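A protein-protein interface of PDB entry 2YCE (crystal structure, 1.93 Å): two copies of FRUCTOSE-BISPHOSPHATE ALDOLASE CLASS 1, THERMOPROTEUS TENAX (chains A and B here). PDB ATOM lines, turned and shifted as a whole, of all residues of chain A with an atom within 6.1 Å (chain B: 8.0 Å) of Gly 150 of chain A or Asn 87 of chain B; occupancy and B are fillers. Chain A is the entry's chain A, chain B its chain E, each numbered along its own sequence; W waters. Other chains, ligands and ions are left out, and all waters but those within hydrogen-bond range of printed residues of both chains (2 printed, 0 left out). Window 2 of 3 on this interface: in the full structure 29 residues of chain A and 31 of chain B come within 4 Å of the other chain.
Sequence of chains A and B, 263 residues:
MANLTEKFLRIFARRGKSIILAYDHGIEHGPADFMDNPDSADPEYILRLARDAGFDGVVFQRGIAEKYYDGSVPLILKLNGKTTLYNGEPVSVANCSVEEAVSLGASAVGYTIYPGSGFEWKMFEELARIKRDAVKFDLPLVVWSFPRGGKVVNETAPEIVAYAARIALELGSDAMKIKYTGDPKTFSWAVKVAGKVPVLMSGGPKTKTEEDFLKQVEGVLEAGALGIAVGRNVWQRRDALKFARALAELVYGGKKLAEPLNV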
ATOM      1  N   GLU A  89     -13.495 -20.313  -7.098  1.00  0.00           N
ATOM      2  CA  GLU A  89     -12.947 -20.178  -5.747  1.00  0.00           C
ATOM      3  C   GLU A  89     -12.435 -18.725  -5.615  1.00  0.00           C
ATOM      4  O   GLU A  89     -11.849 -18.192  -6.553  1.00  0.00           O
ATOM      5  CB  GLU A  89     -11.872 -21.271  -5.488  1.00  0.00           C
ATOM      6  CG  GLU A  89     -12.487 -22.656  -4.902  1.00  0.00           C
ATOM      7  CD  GLU A  89     -12.880 -22.575  -3.408  1.00  0.00           C
ATOM      8  OE1 GLU A  89     -12.016 -22.206  -2.621  1.00  0.00           O
ATOM      9  OE2 GLU A  89     -14.023 -22.912  -2.952  1.00  0.00           O
ATOM     10  N   PRO A  90     -12.721 -18.054  -4.482  1.00  0.00           N
ATOM     11  CA  PRO A  90     -12.456 -16.608  -4.381  1.00  0.00           C
ATOM     12  C   PRO A  90     -11.000 -16.248  -4.634  1.00  0.00           C
ATOM     13  O   PRO A  90     -10.089 -16.869  -4.071  1.00  0.00           O
ATOM     14  CB  PRO A  90     -12.774 -16.270  -2.919  1.00  0.00           C
ATOM     15  CG  PRO A  90     -13.196 -17.552  -2.276  1.00  0.00           C
ATOM     16  CD  PRO A  90     -13.529 -18.531  -3.339  1.00  0.00           C
ATOM     17  N   GLY A 116      -8.533 -20.101   3.033  1.00  0.00           N
ATOM     18  CA  GLY A 116      -9.461 -21.214   2.817  1.00  0.00           C
ATOM     19  C   GLY A 116      -9.779 -21.426   1.349  1.00  0.00           C
ATOM     20  O   GLY A 116     -10.042 -22.551   0.933  1.00  0.00           O
ATOM     21  N   SER A 117      -9.744 -20.351   0.553  1.00  0.00           N
ATOM     22  CA  SER A 117     -10.021 -20.470  -0.901  1.00  0.00           C
ATOM     23  C   SER A 117      -9.113 -21.492  -1.559  1.00  0.00           C
ATOM     24  O   SER A 117      -7.953 -21.638  -1.165  1.00  0.00           O
ATOM     25  CB  SER A 117      -9.852 -19.093  -1.585  1.00  0.00           C
ATOM     26  OG  SER A 117      -9.916 -19.200  -2.987  1.00  0.00           O
ATOM     27  N   GLY A 118      -9.627 -22.206  -2.572  1.00  0.00           N
ATOM     28  CA  GLY A 118      -8.790 -23.079  -3.386  1.00  0.00           C
ATOM     29  C   GLY A 118      -7.633 -22.318  -4.015  1.00  0.00           C
ATOM     30  O   GLY A 118      -6.653 -22.927  -4.436  1.00  0.00           O
ATOM     31  N   ARG A 148     -12.864 -17.247   3.041  1.00  0.00           N
ATOM     32  CA  ARG A 148     -13.942 -17.440   2.076  1.00  0.00           C
ATOM     33  C   ARG A 148     -13.547 -18.620   1.174  1.00  0.00           C
ATOM     34  O   ARG A 148     -12.383 -18.718   0.755  1.00  0.00           O
ATOM     35  CB  ARG A 148     -14.123 -16.169   1.212  1.00  0.00           C
ATOM     36  CG  ARG A 148     -15.467 -16.131   0.458  1.00  0.00           C
ATOM     37  CD  ARG A 148     -15.749 -14.733  -0.126  1.00  0.00           C
ATOM     38  NE  ARG A 148     -16.098 -13.785   0.931  1.00  0.00           N
ATOM     39  CZ  ARG A 148     -16.079 -12.455   0.826  1.00  0.00           C
ATOM     40  NH1 ARG A 148     -15.731 -11.864  -0.309  1.00  0.00           N
ATOM     41  NH2 ARG A 148     -16.432 -11.711   1.875  1.00  0.00           N
ATOM     42  N   GLY A 149     -14.495 -19.505   0.890  1.00  0.00           N
ATOM     43  CA  GLY A 149     -14.200 -20.724   0.123  1.00  0.00           C
ATOM     44  C   GLY A 149     -13.687 -21.825   1.059  1.00  0.00           C
ATOM     45  O   GLY A 149     -13.641 -21.650   2.291  1.00  0.00           O
ATOM     46  N   GLY A 150     -13.295 -22.951   0.495  1.00  0.00           N
ATOM     47  CA  GLY A 150     -12.841 -24.086   1.317  1.00  0.00           C
ATOM     48  C   GLY A 150     -13.871 -24.444   2.364  1.00  0.00           C
ATOM     49  O   GLY A 150     -15.049 -24.659   2.044  1.00  0.00           O
ATOM     50  N   LYS A 151     -13.431 -24.536   3.610  1.00  0.00           N
ATOM     51  CA  LYS A 151     -14.277 -24.997   4.702  1.00  0.00           C
ATOM     52  C   LYS A 151     -15.139 -23.882   5.295  1.00  0.00           C
ATOM     53  O   LYS A 151     -15.948 -24.140   6.205  1.00  0.00           O
ATOM     54  CB  LYS A 151     -13.395 -25.559   5.832  1.00  0.00           C
ATOM     55  CG  LYS A 151     -12.681 -26.860   5.492  1.00  0.00           C
ATOM     56  CD  LYS A 151     -11.874 -27.365   6.661  1.00  0.00           C
ATOM     57  CE  LYS A 151     -11.195 -28.728   6.312  1.00  0.00           C
ATOM     58  NZ  LYS A 151     -10.155 -28.523   5.284  1.00  0.00           N
ATOM     59  N   VAL A 152     -14.930 -22.642   4.849  1.00  0.00           N
ATOM     60  CA  VAL A 152     -15.611 -21.465   5.451  1.00  0.00           C
ATOM     61  C   VAL A 152     -17.104 -21.435   5.085  1.00  0.00           C
ATOM     62  O   VAL A 152     -17.456 -21.400   3.901  1.00  0.00           O
ATOM     63  CB  VAL A 152     -14.943 -20.129   5.016  1.00  0.00           C
ATOM     64  CG1 VAL A 152     -15.644 -18.923   5.688  1.00  0.00           C
ATOM     65  CG2 VAL A 152     -13.428 -20.161   5.390  1.00  0.00           C
ATOM     66  N   VAL A 153     -17.962 -21.473   6.109  1.00  0.00           N
ATOM     67  CA  VAL A 153     -19.420 -21.435   5.888  1.00  0.00           C
ATOM     68  C   VAL A 153     -20.105 -20.257   6.596  1.00  0.00           C
ATOM     69  O   VAL A 153     -21.187 -19.831   6.199  1.00  0.00           O
ATOM     70  CB  VAL A 153     -20.131 -22.756   6.306  1.00  0.00           C
ATOM     71  CG1 VAL A 153     -19.797 -23.933   5.330  1.00  0.00           C
ATOM     72  CG2 VAL A 153     -19.865 -23.113   7.816  1.00  0.00           C
ATOM     73  N   LYS B  82       0.215 -22.506   5.051  1.00  0.00           N
ATOM     74  CA  LYS B  82      -1.152 -22.647   4.533  1.00  0.00           C
ATOM     75  C   LYS B  82      -2.108 -22.738   5.732  1.00  0.00           C
ATOM     76  O   LYS B  82      -1.659 -22.812   6.882  1.00  0.00           O
ATOM     77  CB  LYS B  82      -1.260 -23.915   3.680  1.00  0.00           C
ATOM     78  CG  LYS B  82      -0.982 -25.176   4.504  1.00  0.00           C
ATOM     79  CD  LYS B  82      -1.431 -26.457   3.786  1.00  0.00           C
ATOM     80  CE  LYS B  82      -2.946 -26.677   3.861  1.00  0.00           C
ATOM     81  NZ  LYS B  82      -3.395 -27.334   5.186  1.00  0.00           N
ATOM     82  N   THR B  83      -3.418 -22.790   5.476  1.00  0.00           N
ATOM     83  CA  THR B  83      -4.389 -22.902   6.580  1.00  0.00           C
ATOM     84  C   THR B  83      -5.118 -24.240   6.530  1.00  0.00           C
ATOM     85  O   THR B  83      -5.145 -24.895   5.485  1.00  0.00           O
ATOM     86  CB  THR B  83      -5.454 -21.773   6.487  1.00  0.00           C
ATOM     87  OG1 THR B  83      -6.337 -22.048   5.390  1.00  0.00           O
ATOM     88  CG2 THR B  83      -4.756 -20.359   6.255  1.00  0.00           C
ATOM     89  N   THR B  84      -5.775 -24.624   7.626  1.00  0.00           N
ATOM     90  CA  THR B  84      -6.618 -25.813   7.594  1.00  0.00           C
ATOM     91  C   THR B  84      -7.962 -25.533   6.971  1.00  0.00           C
ATOM     92  O   THR B  84      -8.737 -26.466   6.751  1.00  0.00           O
ATOM     93  CB  THR B  84      -6.914 -26.378   9.017  1.00  0.00           C
ATOM     94  OG1 THR B  84      -7.392 -25.310   9.844  1.00  0.00           O
ATOM     95  CG2 THR B  84      -5.671 -26.967   9.611  1.00  0.00           C
ATOM     96  N   LEU B  85      -8.266 -24.253   6.714  1.00  0.00           N
ATOM     97  CA  LEU B  85      -9.528 -23.874   6.090  1.00  0.00           C
ATOM     98  C   LEU B  85      -9.536 -24.313   4.632  1.00  0.00           C
ATOM     99  O   LEU B  85     -10.596 -24.542   4.044  1.00  0.00           O
ATOM    100  CB  LEU B  85      -9.709 -22.347   6.165  1.00  0.00           C
ATOM    101  CG  LEU B  85      -9.896 -21.729   7.564  1.00  0.00           C
ATOM    102  CD1 LEU B  85      -9.901 -20.227   7.380  1.00  0.00           C
ATOM    103  CD2 LEU B  85     -11.208 -22.172   8.199  1.00  0.00           C
ATOM    104  N   TYR B  86      -8.326 -24.395   4.079  1.00  0.00           N
ATOM    105  CA  TYR B  86      -8.097 -24.783   2.702  1.00  0.00           C
ATOM    106  C   TYR B  86      -8.535 -26.240   2.459  1.00  0.00           C
ATOM    107  O   TYR B  86      -8.172 -27.143   3.233  1.00  0.00           O
ATOM    108  CB  TYR B  86      -6.599 -24.589   2.396  1.00  0.00           C
ATOM    109  CG  TYR B  86      -6.155 -25.114   1.059  1.00  0.00           C
ATOM    110  CD1 TYR B  86      -6.462 -24.428  -0.125  1.00  0.00           C
ATOM    111  CD2 TYR B  86      -5.416 -26.310   0.967  1.00  0.00           C
ATOM    112  CE1 TYR B  86      -6.042 -24.929  -1.389  1.00  0.00           C
ATOM    113  CE2 TYR B  86      -4.984 -26.826  -0.292  1.00  0.00           C
ATOM    114  CZ  TYR B  86      -5.289 -26.120  -1.460  1.00  0.00           C
ATOM    115  OH  TYR B  86      -4.889 -26.627  -2.686  1.00  0.00           O
ATOM    116  N   ASN B  87      -9.280 -26.458   1.379  1.00  0.00           N
ATOM    117  CA  ASN B  87      -9.697 -27.786   0.954  1.00  0.00           C
ATOM    118  C   ASN B  87      -8.988 -28.452  -0.249  1.00  0.00           C
ATOM    119  O   ASN B  87      -9.274 -29.616  -0.530  1.00  0.00           O
ATOM    120  CB  ASN B  87     -11.189 -27.765   0.582  1.00  0.00           C
ATOM    121  CG  ASN B  87     -12.094 -27.997   1.763  1.00  0.00           C
ATOM    122  OD1 ASN B  87     -11.673 -28.561   2.779  1.00  0.00           O
ATOM    123  ND2 ASN B  87     -13.356 -27.589   1.629  1.00  0.00           N
ATOM    124  N   GLY B  88      -8.180 -27.782  -1.049  1.00  0.00           N
ATOM    125  CA  GLY B  88      -7.546 -28.599  -2.161  1.00  0.00           C
ATOM    126  C   GLY B  88      -6.458 -29.661  -1.860  1.00  0.00           C
ATOM    127  O   GLY B  88      -6.206 -30.040  -0.680  1.00  0.00           O
ATOM    128  N   GLU B  89      -5.821 -30.184  -2.930  1.00  0.00           N
ATOM    129  CA  GLU B  89      -4.576 -30.943  -2.766  1.00  0.00           C
ATOM    130  C   GLU B  89      -3.553 -30.034  -1.986  1.00  0.00           C
ATOM    131  O   GLU B  89      -3.427 -28.841  -2.261  1.00  0.00           O
ATOM    132  CB  GLU B  89      -4.052 -31.503  -4.121  1.00  0.00           C
ATOM    133  CG  GLU B  89      -4.648 -32.961  -4.602  1.00  0.00           C
ATOM    134  CD  GLU B  89      -4.226 -34.243  -3.744  1.00  0.00           C
ATOM    135  OE1 GLU B  89      -3.050 -34.468  -3.458  1.00  0.00           O
ATOM    136  OE2 GLU B  89      -5.066 -35.104  -3.366  1.00  0.00           O
ATOM    137  N   PRO B  90      -2.861 -30.591  -0.979  1.00  0.00           N
ATOM    138  CA  PRO B  90      -2.052 -29.816  -0.037  1.00  0.00           C
ATOM    139  C   PRO B  90      -0.975 -28.993  -0.748  1.00  0.00           C
ATOM    140  O   PRO B  90      -0.249 -29.517  -1.582  1.00  0.00           O
ATOM    141  CB  PRO B  90      -1.363 -30.900   0.795  1.00  0.00           C
ATOM    142  CG  PRO B  90      -2.271 -32.038   0.711  1.00  0.00           C
ATOM    143  CD  PRO B  90      -2.814 -32.032  -0.658  1.00  0.00           C
HETATM  144  O   HOH W   1     -10.168 -24.836  -0.649  1.00  0.00           O
HETATM  145  O   HOH W   2      -5.604 -25.310  -5.196  1.00  0.00           O
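ND2 of Asn 87 of chain B sits close to O of Gly 150 of chain A (3.4 Å).
NZ of Lys 151 of chain A is in hydrogen-bond range of O of Thr 84 of chain B, 2.9 Å away.
The backbone carbonyl oxygen (O) of Leu 85 of chain B lies within hydrogen-bond range of the backbone NH (N) of Lys 151 of chain A, 2.9 Å away.
O of Tyr 86 of chain B is in hydrogen-bond range of NZ of Lys 151 of chain A, at 3.2 Å.
The side-chain amino group of Lys 151 of chain A sits at hydrogen-bond distance from the side-chain amide oxygen of Asn 87 of chain B (2.9 Å).
The side-chain carboxylate of Glu 89 of chain A sits at hydrogen-bond distance from the backbone NH of Gly 150 of chain A (3.4 Å).
The backbone carbonyl oxygen (O) of Gly 116 of chain A sits close to the backbone NH (N) of Gly 150 of chain A, 3.3 Å away.
O of Arg 148 of chain A sits at hydrogen-bond distance from N of Ser 117 of chain A.
The side-chain hydroxyl of Thr 83 of chain B sits close to the backbone NH of Leu 85 of chain B (3.2 Å).
The side-chain hydroxyl of Thr 83 of chain B is in hydrogen-bond range of the backbone NH of Tyr 86 of chain B (3.3 Å).
OH of Tyr 86 of chain B sits at hydrogen-bond distance from O of Glu 89 of chain B (2.7 Å).
Thr 83 of chain B touches Gly 116 of chain A.
Gly 116 of chain A touches Leu 85 of chain B (CA to CB, 3.5 Å).
CA of Tyr 86 of chain B touches O of Gly 116 of chain A (3.4 Å).
Ser 117 of chain A touches Tyr 86 of chain B (O to CD1, 3.3 Å).
Gly 118 of chain A touches Tyr 86 of chain B.
Gly 150 of chain A touches Leu 85 of chain B.
Pro 90 of chain A touches none of the printed residues of chain B.
Of the printed residues of chain B, Gly 116 of chain A touches Thr 83, Leu 85 and Tyr 86.
No residue of chain B comes within 4 Å of Gly 149 of chain A.
Of chain B, only Leu 85 and Asn 87 come within 4 Å of Gly 150 of chain A.
Of the printed residues of chain B, Lys 151 of chain A touches Thr 84, Leu 85, Tyr 86 and Asn 87.
Of the printed residues of chain A, Thr 84 of chain B touches Lys 151 (2.9 Å).
Of the printed residues of chain A, Tyr 86 of chain B touches Gly 116 (3.4 Å), Ser 117 (3.3 Å), Gly 118 (3.7 Å) and Lys 151 (3.2 Å).
The nearest printed residue of chain A that does not touch Asn 87 of chain B is Gly 116 of chain A (4.01 Å).
Of the 11 printed residues of chain A, 5 touch a printed residue of chain B.
Printed residues of chain A that touch a printed residue of chain B: Gly 116, Ser 117, Gly 118, Gly 150 and Lys 151.
Hydrophobic or aromatic side chains of chain B that line the printed part of chain A: Leu 85 and Tyr 86.
Among the printed residues, 11 pairs touch across the chains.
Among the printed residues, no Asp or Glu carboxylate lies within 4 Å of a Lys or Arg side-chain nitrogen of the other chain.
2 positions are printed for both chains.
Of the 11 pairs that touch across the chains among the printed residues, none has its exchanged pair printed and touching as well.
Water W2 lies within hydrogen-bond range of O of Gly 118 of chain A (2.7 Å) and OH of Tyr 86 of chain B (2.9 Å).
Water W1 lies within hydrogen-bond range of N of Asn 87 of chain B (2.7 Å), O of Gly 116 of chain A (2.8 Å) and N of Gly 118 of chain A (3.3 Å).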
